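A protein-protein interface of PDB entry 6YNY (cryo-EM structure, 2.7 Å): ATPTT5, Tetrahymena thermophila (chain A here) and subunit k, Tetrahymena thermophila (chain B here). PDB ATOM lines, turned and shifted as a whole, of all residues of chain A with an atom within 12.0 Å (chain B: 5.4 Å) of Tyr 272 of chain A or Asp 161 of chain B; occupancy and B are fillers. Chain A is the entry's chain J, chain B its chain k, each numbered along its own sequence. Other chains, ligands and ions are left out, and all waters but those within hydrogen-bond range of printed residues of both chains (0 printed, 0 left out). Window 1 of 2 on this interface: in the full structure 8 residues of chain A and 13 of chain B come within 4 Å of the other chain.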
ATOM      1  N   ASP A 215      -9.486   8.150  12.617  1.00  0.00           N
ATOM      2  CA  ASP A 215      -9.491   7.824  11.194  1.00  0.00           C
ATOM      3  C   ASP A 215     -10.891   7.958  10.600  1.00  0.00           C
ATOM      4  O   ASP A 215     -11.418   7.038   9.977  1.00  0.00           O
ATOM      5  CB  ASP A 215      -8.939   6.422  10.982  1.00  0.00           C
ATOM      6  CG  ASP A 215      -8.655   6.120   9.528  1.00  0.00           C
ATOM      7  OD1 ASP A 215      -8.874   7.011   8.682  1.00  0.00           O
ATOM      8  OD2 ASP A 215      -8.212   4.993   9.229  1.00  0.00           O
ATOM      9  N   THR A 216     -11.504   9.121  10.803  1.00  0.00           N
ATOM     10  CA  THR A 216     -12.805   9.431  10.233  1.00  0.00           C
ATOM     11  C   THR A 216     -12.784  10.858   9.711  1.00  0.00           C
ATOM     12  O   THR A 216     -12.064  11.714  10.231  1.00  0.00           O
ATOM     13  CB  THR A 216     -13.930   9.256  11.258  1.00  0.00           C
ATOM     14  OG1 THR A 216     -13.658  10.053  12.415  1.00  0.00           O
ATOM     15  CG2 THR A 216     -14.049   7.806  11.668  1.00  0.00           C
ATOM     16  N   LYS A 242      -1.974   4.184  -7.725  1.00  0.00           N
ATOM     17  CA  LYS A 242      -2.436   2.832  -8.005  1.00  0.00           C
ATOM     18  C   LYS A 242      -1.841   2.267  -9.285  1.00  0.00           C
ATOM     19  O   LYS A 242      -1.939   1.054  -9.509  1.00  0.00           O
ATOM     20  CB  LYS A 242      -3.961   2.809  -8.079  1.00  0.00           C
ATOM     21  CG  LYS A 242      -4.623   3.030  -6.732  1.00  0.00           C
ATOM     22  CD  LYS A 242      -6.128   3.183  -6.846  1.00  0.00           C
ATOM     23  CE  LYS A 242      -6.790   1.885  -7.256  1.00  0.00           C
ATOM     24  NZ  LYS A 242      -8.272   1.978  -7.168  1.00  0.00           N
ATOM     25  N   VAL A 267     -12.029 -21.623   9.165  1.00  0.00           N
ATOM     26  CA  VAL A 267     -11.246 -20.552   8.563  1.00  0.00           C
ATOM     27  C   VAL A 267     -11.955 -19.221   8.773  1.00  0.00           C
ATOM     28  O   VAL A 267     -13.185 -19.157   8.905  1.00  0.00           O
ATOM     29  CB  VAL A 267     -11.011 -20.830   7.067  1.00  0.00           C
ATOM     30  CG1 VAL A 267     -12.311 -20.722   6.293  1.00  0.00           C
ATOM     31  CG2 VAL A 267      -9.976 -19.879   6.506  1.00  0.00           C
ATOM     32  N   GLU A 268     -11.173 -18.145   8.811  1.00  0.00           N
ATOM     33  CA  GLU A 268     -11.746 -16.820   9.006  1.00  0.00           C
ATOM     34  C   GLU A 268     -12.797 -16.541   7.940  1.00  0.00           C
ATOM     35  O   GLU A 268     -12.561 -16.745   6.747  1.00  0.00           O
ATOM     36  CB  GLU A 268     -10.652 -15.750   8.975  1.00  0.00           C
ATOM     37  CG  GLU A 268      -9.979 -15.524   7.618  1.00  0.00           C
ATOM     38  CD  GLU A 268      -9.113 -16.687   7.177  1.00  0.00           C
ATOM     39  OE1 GLU A 268      -8.744 -16.737   5.985  1.00  0.00           O
ATOM     40  OE2 GLU A 268      -8.803 -17.553   8.021  1.00  0.00           O
ATOM     41  N   LYS A 269     -13.966 -16.086   8.380  1.00  0.00           N
ATOM     42  CA  LYS A 269     -15.049 -15.803   7.454  1.00  0.00           C
ATOM     43  C   LYS A 269     -14.769 -14.526   6.673  1.00  0.00           C
ATOM     44  O   LYS A 269     -14.063 -13.627   7.136  1.00  0.00           O
ATOM     45  CB  LYS A 269     -16.372 -15.677   8.203  1.00  0.00           C
ATOM     46  CG  LYS A 269     -16.922 -17.001   8.698  1.00  0.00           C
ATOM     47  CD  LYS A 269     -18.134 -16.819   9.596  1.00  0.00           C
ATOM     48  CE  LYS A 269     -19.306 -16.204   8.844  1.00  0.00           C
ATOM     49  NZ  LYS A 269     -20.522 -16.102   9.700  1.00  0.00           N
ATOM     50  N   SER A 270     -15.330 -14.457   5.471  1.00  0.00           N
ATOM     51  CA  SER A 270     -15.189 -13.265   4.656  1.00  0.00           C
ATOM     52  C   SER A 270     -15.970 -12.113   5.272  1.00  0.00           C
ATOM     53  O   SER A 270     -16.995 -12.309   5.929  1.00  0.00           O
ATOM     54  CB  SER A 270     -15.674 -13.531   3.234  1.00  0.00           C
ATOM     55  OG  SER A 270     -14.875 -14.516   2.604  1.00  0.00           O
ATOM     56  N   LEU A 271     -15.471 -10.896   5.057  1.00  0.00           N
ATOM     57  CA  LEU A 271     -16.130  -9.724   5.617  1.00  0.00           C
ATOM     58  C   LEU A 271     -17.570  -9.628   5.140  1.00  0.00           C
ATOM     59  O   LEU A 271     -18.460  -9.227   5.898  1.00  0.00           O
ATOM     60  CB  LEU A 271     -15.369  -8.460   5.231  1.00  0.00           C
ATOM     61  CG  LEU A 271     -13.880  -8.433   5.546  1.00  0.00           C
ATOM     62  CD1 LEU A 271     -13.288  -7.128   5.082  1.00  0.00           C
ATOM     63  CD2 LEU A 271     -13.661  -8.621   7.019  1.00  0.00           C
ATOM     64  N   TYR A 272     -17.816  -9.997   3.890  1.00  0.00           N
ATOM     65  CA  TYR A 272     -19.118  -9.863   3.267  1.00  0.00           C
ATOM     66  C   TYR A 272     -19.508 -11.167   2.590  1.00  0.00           C
ATOM     67  O   TYR A 272     -18.642 -11.912   2.120  1.00  0.00           O
ATOM     68  CB  TYR A 272     -19.108  -8.725   2.242  1.00  0.00           C
ATOM     69  CG  TYR A 272     -18.620  -7.419   2.817  1.00  0.00           C
ATOM     70  CD1 TYR A 272     -17.344  -6.955   2.547  1.00  0.00           C
ATOM     71  CD2 TYR A 272     -19.430  -6.659   3.645  1.00  0.00           C
ATOM     72  CE1 TYR A 272     -16.895  -5.766   3.074  1.00  0.00           C
ATOM     73  CE2 TYR A 272     -18.988  -5.471   4.177  1.00  0.00           C
ATOM     74  CZ  TYR A 272     -17.719  -5.030   3.889  1.00  0.00           C
ATOM     75  OH  TYR A 272     -17.270  -3.846   4.414  1.00  0.00           O
ATOM     76  N   PRO A 273     -20.812 -11.468   2.522  1.00  0.00           N
ATOM     77  CA  PRO A 273     -21.289 -12.745   1.981  1.00  0.00           C
ATOM     78  C   PRO A 273     -20.921 -12.958   0.516  1.00  0.00           C
ATOM     79  O   PRO A 273     -20.107 -13.836   0.224  1.00  0.00           O
ATOM     80  CB  PRO A 273     -22.809 -12.646   2.152  1.00  0.00           C
ATOM     81  CG  PRO A 273     -23.093 -11.200   2.209  1.00  0.00           C
ATOM     82  CD  PRO A 273     -21.928 -10.584   2.893  1.00  0.00           C
ATOM     83  N   VAL B 107     -19.909   2.398  -3.873  1.00  0.00           N
ATOM     84  CA  VAL B 107     -20.320   1.088  -4.350  1.00  0.00           C
ATOM     85  C   VAL B 107     -21.115   1.300  -5.631  1.00  0.00           C
ATOM     86  O   VAL B 107     -21.643   2.383  -5.898  1.00  0.00           O
ATOM     87  CB  VAL B 107     -21.143   0.305  -3.310  1.00  0.00           C
ATOM     88  CG1 VAL B 107     -20.452   0.319  -1.968  1.00  0.00           C
ATOM     89  CG2 VAL B 107     -22.535   0.870  -3.195  1.00  0.00           C
ATOM     90  N   TYR B 139     -29.562  -5.074   0.993  1.00  0.00           N
ATOM     91  CA  TYR B 139     -28.488  -5.467   1.896  1.00  0.00           C
ATOM     92  C   TYR B 139     -28.598  -4.651   3.176  1.00  0.00           C
ATOM     93  O   TYR B 139     -28.302  -3.453   3.184  1.00  0.00           O
ATOM     94  CB  TYR B 139     -27.135  -5.256   1.224  1.00  0.00           C
ATOM     95  CG  TYR B 139     -25.969  -5.932   1.907  1.00  0.00           C
ATOM     96  CD1 TYR B 139     -26.152  -6.744   3.014  1.00  0.00           C
ATOM     97  CD2 TYR B 139     -24.679  -5.748   1.443  1.00  0.00           C
ATOM     98  CE1 TYR B 139     -25.086  -7.357   3.631  1.00  0.00           C
ATOM     99  CE2 TYR B 139     -23.608  -6.355   2.056  1.00  0.00           C
ATOM    100  CZ  TYR B 139     -23.816  -7.158   3.150  1.00  0.00           C
ATOM    101  OH  TYR B 139     -22.748  -7.766   3.763  1.00  0.00           O
ATOM    102  N   HIS B 141     -26.862  -4.525   5.844  1.00  0.00           N
ATOM    103  CA  HIS B 141     -25.634  -3.952   6.380  1.00  0.00           C
ATOM    104  C   HIS B 141     -25.266  -2.664   5.655  1.00  0.00           C
ATOM    105  O   HIS B 141     -24.960  -1.649   6.289  1.00  0.00           O
ATOM    106  CB  HIS B 141     -24.494  -4.961   6.281  1.00  0.00           C
ATOM    107  CG  HIS B 141     -23.181  -4.424   6.751  1.00  0.00           C
ATOM    108  ND1 HIS B 141     -22.964  -4.025   8.050  1.00  0.00           N
ATOM    109  CD2 HIS B 141     -22.022  -4.201   6.089  1.00  0.00           C
ATOM    110  CE1 HIS B 141     -21.723  -3.588   8.173  1.00  0.00           C
ATOM    111  NE2 HIS B 141     -21.130  -3.684   6.997  1.00  0.00           N
ATOM    112  N   TRP B 156     -12.836   6.399   4.713  1.00  0.00           N
ATOM    113  CA  TRP B 156     -12.423   5.870   3.428  1.00  0.00           C
ATOM    114  C   TRP B 156     -12.751   4.385   3.338  1.00  0.00           C
ATOM    115  O   TRP B 156     -12.910   3.692   4.346  1.00  0.00           O
ATOM    116  CB  TRP B 156     -10.930   6.102   3.203  1.00  0.00           C
ATOM    117  CG  TRP B 156     -10.058   5.523   4.261  1.00  0.00           C
ATOM    118  CD1 TRP B 156      -9.660   6.128   5.413  1.00  0.00           C
ATOM    119  CD2 TRP B 156      -9.464   4.222   4.266  1.00  0.00           C
ATOM    120  NE1 TRP B 156      -8.859   5.285   6.139  1.00  0.00           N
ATOM    121  CE2 TRP B 156      -8.723   4.107   5.455  1.00  0.00           C
ATOM    122  CE3 TRP B 156      -9.490   3.144   3.380  1.00  0.00           C
ATOM    123  CZ2 TRP B 156      -8.015   2.958   5.781  1.00  0.00           C
ATOM    124  CZ3 TRP B 156      -8.786   2.004   3.705  1.00  0.00           C
ATOM    125  CH2 TRP B 156      -8.059   1.919   4.895  1.00  0.00           C
ATOM    126  N   MET B 157     -12.850   3.899   2.106  1.00  0.00           N
ATOM    127  CA  MET B 157     -13.253   2.531   1.831  1.00  0.00           C
ATOM    128  C   MET B 157     -12.164   1.815   1.050  1.00  0.00           C
ATOM    129  O   MET B 157     -11.584   2.374   0.114  1.00  0.00           O
ATOM    130  CB  MET B 157     -14.563   2.499   1.043  1.00  0.00           C
ATOM    131  CG  MET B 157     -15.723   3.130   1.774  1.00  0.00           C
ATOM    132  SD  MET B 157     -17.237   3.216   0.807  1.00  0.00           S
ATOM    133  CE  MET B 157     -17.530   1.487   0.501  1.00  0.00           C
ATOM    134  N   SER B 158     -11.892   0.576   1.444  1.00  0.00           N
ATOM    135  CA  SER B 158     -10.932  -0.257   0.745  1.00  0.00           C
ATOM    136  C   SER B 158     -11.578  -0.873  -0.492  1.00  0.00           C
ATOM    137  O   SER B 158     -12.777  -0.723  -0.744  1.00  0.00           O
ATOM    138  CB  SER B 158     -10.405  -1.343   1.675  1.00  0.00           C
ATOM    139  OG  SER B 158     -11.452  -2.192   2.101  1.00  0.00           O
ATOM    140  N   GLU B 159     -10.768  -1.579  -1.280  1.00  0.00           N
ATOM    141  CA  GLU B 159     -11.305  -2.263  -2.449  1.00  0.00           C
ATOM    142  C   GLU B 159     -12.271  -3.363  -2.047  1.00  0.00           C
ATOM    143  O   GLU B 159     -13.219  -3.657  -2.784  1.00  0.00           O
ATOM    144  CB  GLU B 159     -10.166  -2.836  -3.289  1.00  0.00           C
ATOM    145  CG  GLU B 159      -9.183  -1.793  -3.786  1.00  0.00           C
ATOM    146  CD  GLU B 159      -9.820  -0.788  -4.728  1.00  0.00           C
ATOM    147  OE1 GLU B 159     -10.969  -1.018  -5.160  1.00  0.00           O
ATOM    148  OE2 GLU B 159      -9.169   0.231  -5.038  1.00  0.00           O
ATOM    149  N   LYS B 160     -12.054  -3.972  -0.884  1.00  0.00           N
ATOM    150  CA  LYS B 160     -12.932  -5.036  -0.421  1.00  0.00           C
ATOM    151  C   LYS B 160     -14.256  -4.488   0.092  1.00  0.00           C
ATOM    152  O   LYS B 160     -15.292  -5.142  -0.058  1.00  0.00           O
ATOM    153  CB  LYS B 160     -12.226  -5.839   0.669  1.00  0.00           C
ATOM    154  CG  LYS B 160     -12.905  -7.140   1.019  1.00  0.00           C
ATOM    155  CD  LYS B 160     -12.079  -7.957   1.999  1.00  0.00           C
ATOM    156  CE  LYS B 160     -10.780  -8.450   1.382  1.00  0.00           C
ATOM    157  NZ  LYS B 160     -10.996  -9.202   0.117  1.00  0.00           N
ATOM    158  N   ASP B 161     -14.240  -3.301   0.699  1.00  0.00           N
ATOM    159  CA  ASP B 161     -15.480  -2.684   1.153  1.00  0.00           C
ATOM    160  C   ASP B 161     -16.311  -2.184  -0.019  1.00  0.00           C
ATOM    161  O   ASP B 161     -17.545  -2.200   0.044  1.00  0.00           O
ATOM    162  CB  ASP B 161     -15.175  -1.534   2.108  1.00  0.00           C
ATOM    163  CG  ASP B 161     -14.523  -1.997   3.391  1.00  0.00           C
ATOM    164  OD1 ASP B 161     -14.738  -3.163   3.779  1.00  0.00           O
ATOM    165  OD2 ASP B 161     -13.797  -1.195   4.013  1.00  0.00           O
ATOM    166  N   LYS B 162     -15.656  -1.732  -1.089  1.00  0.00           N
ATOM    167  CA  LYS B 162     -16.382  -1.239  -2.252  1.00  0.00           C
ATOM    168  C   LYS B 162     -17.223  -2.327  -2.901  1.00  0.00           C
ATOM    169  O   LYS B 162     -18.244  -2.027  -3.530  1.00  0.00           O
ATOM    170  CB  LYS B 162     -15.402  -0.667  -3.272  1.00  0.00           C
ATOM    171  CG  LYS B 162     -14.872   0.700  -2.924  1.00  0.00           C
ATOM    172  CD  LYS B 162     -13.915   1.203  -3.980  1.00  0.00           C
ATOM    173  CE  LYS B 162     -13.713   2.695  -3.868  1.00  0.00           C
ATOM    174  NZ  LYS B 162     -13.237   3.081  -2.517  1.00  0.00           N
ATOM    175  N   ASN B 163     -16.819  -3.587  -2.763  1.00  0.00           N
ATOM    176  CA  ASN B 163     -17.522  -4.704  -3.373  1.00  0.00           C
ATOM    177  C   ASN B 163     -18.469  -5.400  -2.406  1.00  0.00           C
ATOM    178  O   ASN B 163     -18.883  -6.535  -2.666  1.00  0.00           O
ATOM    179  CB  ASN B 163     -16.514  -5.705  -3.933  1.00  0.00           C
ATOM    180  CG  ASN B 163     -15.654  -5.113  -5.025  1.00  0.00           C
ATOM    181  OD1 ASN B 163     -16.096  -4.255  -5.786  1.00  0.00           O
ATOM    182  ND2 ASN B 163     -14.414  -5.572  -5.109  1.00  0.00           N
ATOM    183  N   MET B 164     -18.831  -4.743  -1.303  1.00  0.00           N
ATOM    184  CA  MET B 164     -19.717  -5.369  -0.330  1.00  0.00           C
ATOM    185  C   MET B 164     -21.010  -5.849  -0.974  1.00  0.00           C
ATOM    186  O   MET B 164     -21.596  -6.841  -0.527  1.00  0.00           O
ATOM    187  CB  MET B 164     -20.032  -4.393   0.803  1.00  0.00           C
ATOM    188  CG  MET B 164     -20.751  -3.135   0.365  1.00  0.00           C
ATOM    189  SD  MET B 164     -21.477  -2.227   1.739  1.00  0.00           S
ATOM    190  CE  MET B 164     -20.014  -1.818   2.673  1.00  0.00           C
ATOM    191  N   VAL B 165     -21.471  -5.161  -2.017  1.00  0.00           N
ATOM    192  CA  VAL B 165     -22.705  -5.559  -2.682  1.00  0.00           C
ATOM    193  C   VAL B 165     -22.458  -6.722  -3.631  1.00  0.00           C
ATOM    194  O   VAL B 165     -23.314  -7.598  -3.791  1.00  0.00           O
ATOM    195  CB  VAL B 165     -23.319  -4.355  -3.413  1.00  0.00           C
ATOM    196  CG1 VAL B 165     -24.651  -4.732  -4.020  1.00  0.00           C
ATOM    197  CG2 VAL B 165     -23.481  -3.195  -2.463  1.00  0.00           C
ATOM    198  N   TYR B 167     -20.397  -9.138  -3.166  1.00  0.00           N
ATOM    199  CA  TYR B 167     -20.418 -10.325  -2.321  1.00  0.00           C
ATOM    200  C   TYR B 167     -21.846 -10.717  -1.970  1.00  0.00           C
ATOM    201  O   TYR B 167     -22.173 -11.907  -1.897  1.00  0.00           O
ATOM    202  CB  TYR B 167     -19.602 -10.075  -1.055  1.00  0.00           C
ATOM    203  CG  TYR B 167     -18.111 -10.032  -1.284  1.00  0.00           C
ATOM    204  CD1 TYR B 167     -17.369 -11.199  -1.370  1.00  0.00           C
ATOM    205  CD2 TYR B 167     -17.443  -8.825  -1.405  1.00  0.00           C
ATOM    206  CE1 TYR B 167     -16.009 -11.165  -1.576  1.00  0.00           C
ATOM    207  CE2 TYR B 167     -16.085  -8.781  -1.611  1.00  0.00           C
ATOM    208  CZ  TYR B 167     -15.371  -9.952  -1.694  1.00  0.00           C
ATOM    209  OH  TYR B 167     -14.014  -9.909  -1.902  1.00  0.00           O
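OD1 of Asp 215 of chain A lies within hydrogen-bond range of NE1 of Trp 156 of chain B (3.1 Å). The side-chain hydroxyl of Tyr 272 of chain A lies within hydrogen-bond range of the side-chain carboxylate of Asp 161 of chain B (2.7 Å). NZ of Lys 242 of chain A lies within salt-bridge range of OE2 of Glu 159 of chain B (2.9 Å).
Printed residues of chain A that touch a printed residue of chain B: Asp 215, Lys 242, Leu 271, Tyr 272 and Pro 273.
Among the printed residues, pairs that only touch across the chains: Leu 271 of chain A with Lys 160 of chain B (3.4 Å), Tyr 272 of chain A with Tyr 139 of chain B (3.5 Å), Tyr 272 of chain A with His 141 of chain B (3.8 Å), Tyr 272 of chain A with Lys 160 of chain B (3.6 Å), Tyr 272 of chain A with Met 164 of chain B (3.7 Å), Tyr 272 of chain A with Tyr 167 of chain B (3.6 Å), Pro 273 of chain A with Tyr 139 of chain B (3.1 Å) and Pro 273 of chain A with Tyr 167 of chain B (2.9 Å).
The backbone carbonyl oxygen (O) of Glu 159 of chain B lies within hydrogen-bond range of the side-chain amide nitrogen (ND2) of Asn 163 of chain B, at 3.2 Å. The side-chain hydroxyl (OG) of Ser 158 of chain B lies within hydrogen-bond range of the side-chain carboxylate (OD2) of Asp 161 of chain B (3.2 Å).
Of chain B, only Tyr 139, His 141, Lys 160, Asp 161, Met 164 and Tyr 167 come within 4 Å of Tyr 272 of chain A. Asp 161 of chain B touches one residue of chain A. Met 157 of chain B touches none of the printed residues of chain A. Of the printed residues of chain A, Lys 160 of chain B touches Leu 271 and Tyr 272. No residue of chain A comes within 4 Å of Lys 162 of chain B. Of the printed residues of chain A, Met 164 of chain B touches Tyr 272. Tyr 167 of chain B touches just these residues of chain A: Tyr 272 (3.6 Å) and Pro 273 (2.9 Å). Printed residues of chain B within 4 Å of Leu 271 of chain A: Lys 160 (3.4 Å). Of the printed residues of chain A, Trp 156 of chain B touches Asp 215 (3.1 Å). Of the printed residues of chain B, Lys 242 of chain A touches Glu 159. Printed residues of chain A within 4 Å of His 141 of chain B: Tyr 272. Of the printed residues of chain B, Asp 215 of chain A touches Trp 156 (3.1 Å). Glu 268 of chain A touches none of the printed residues of chain B.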
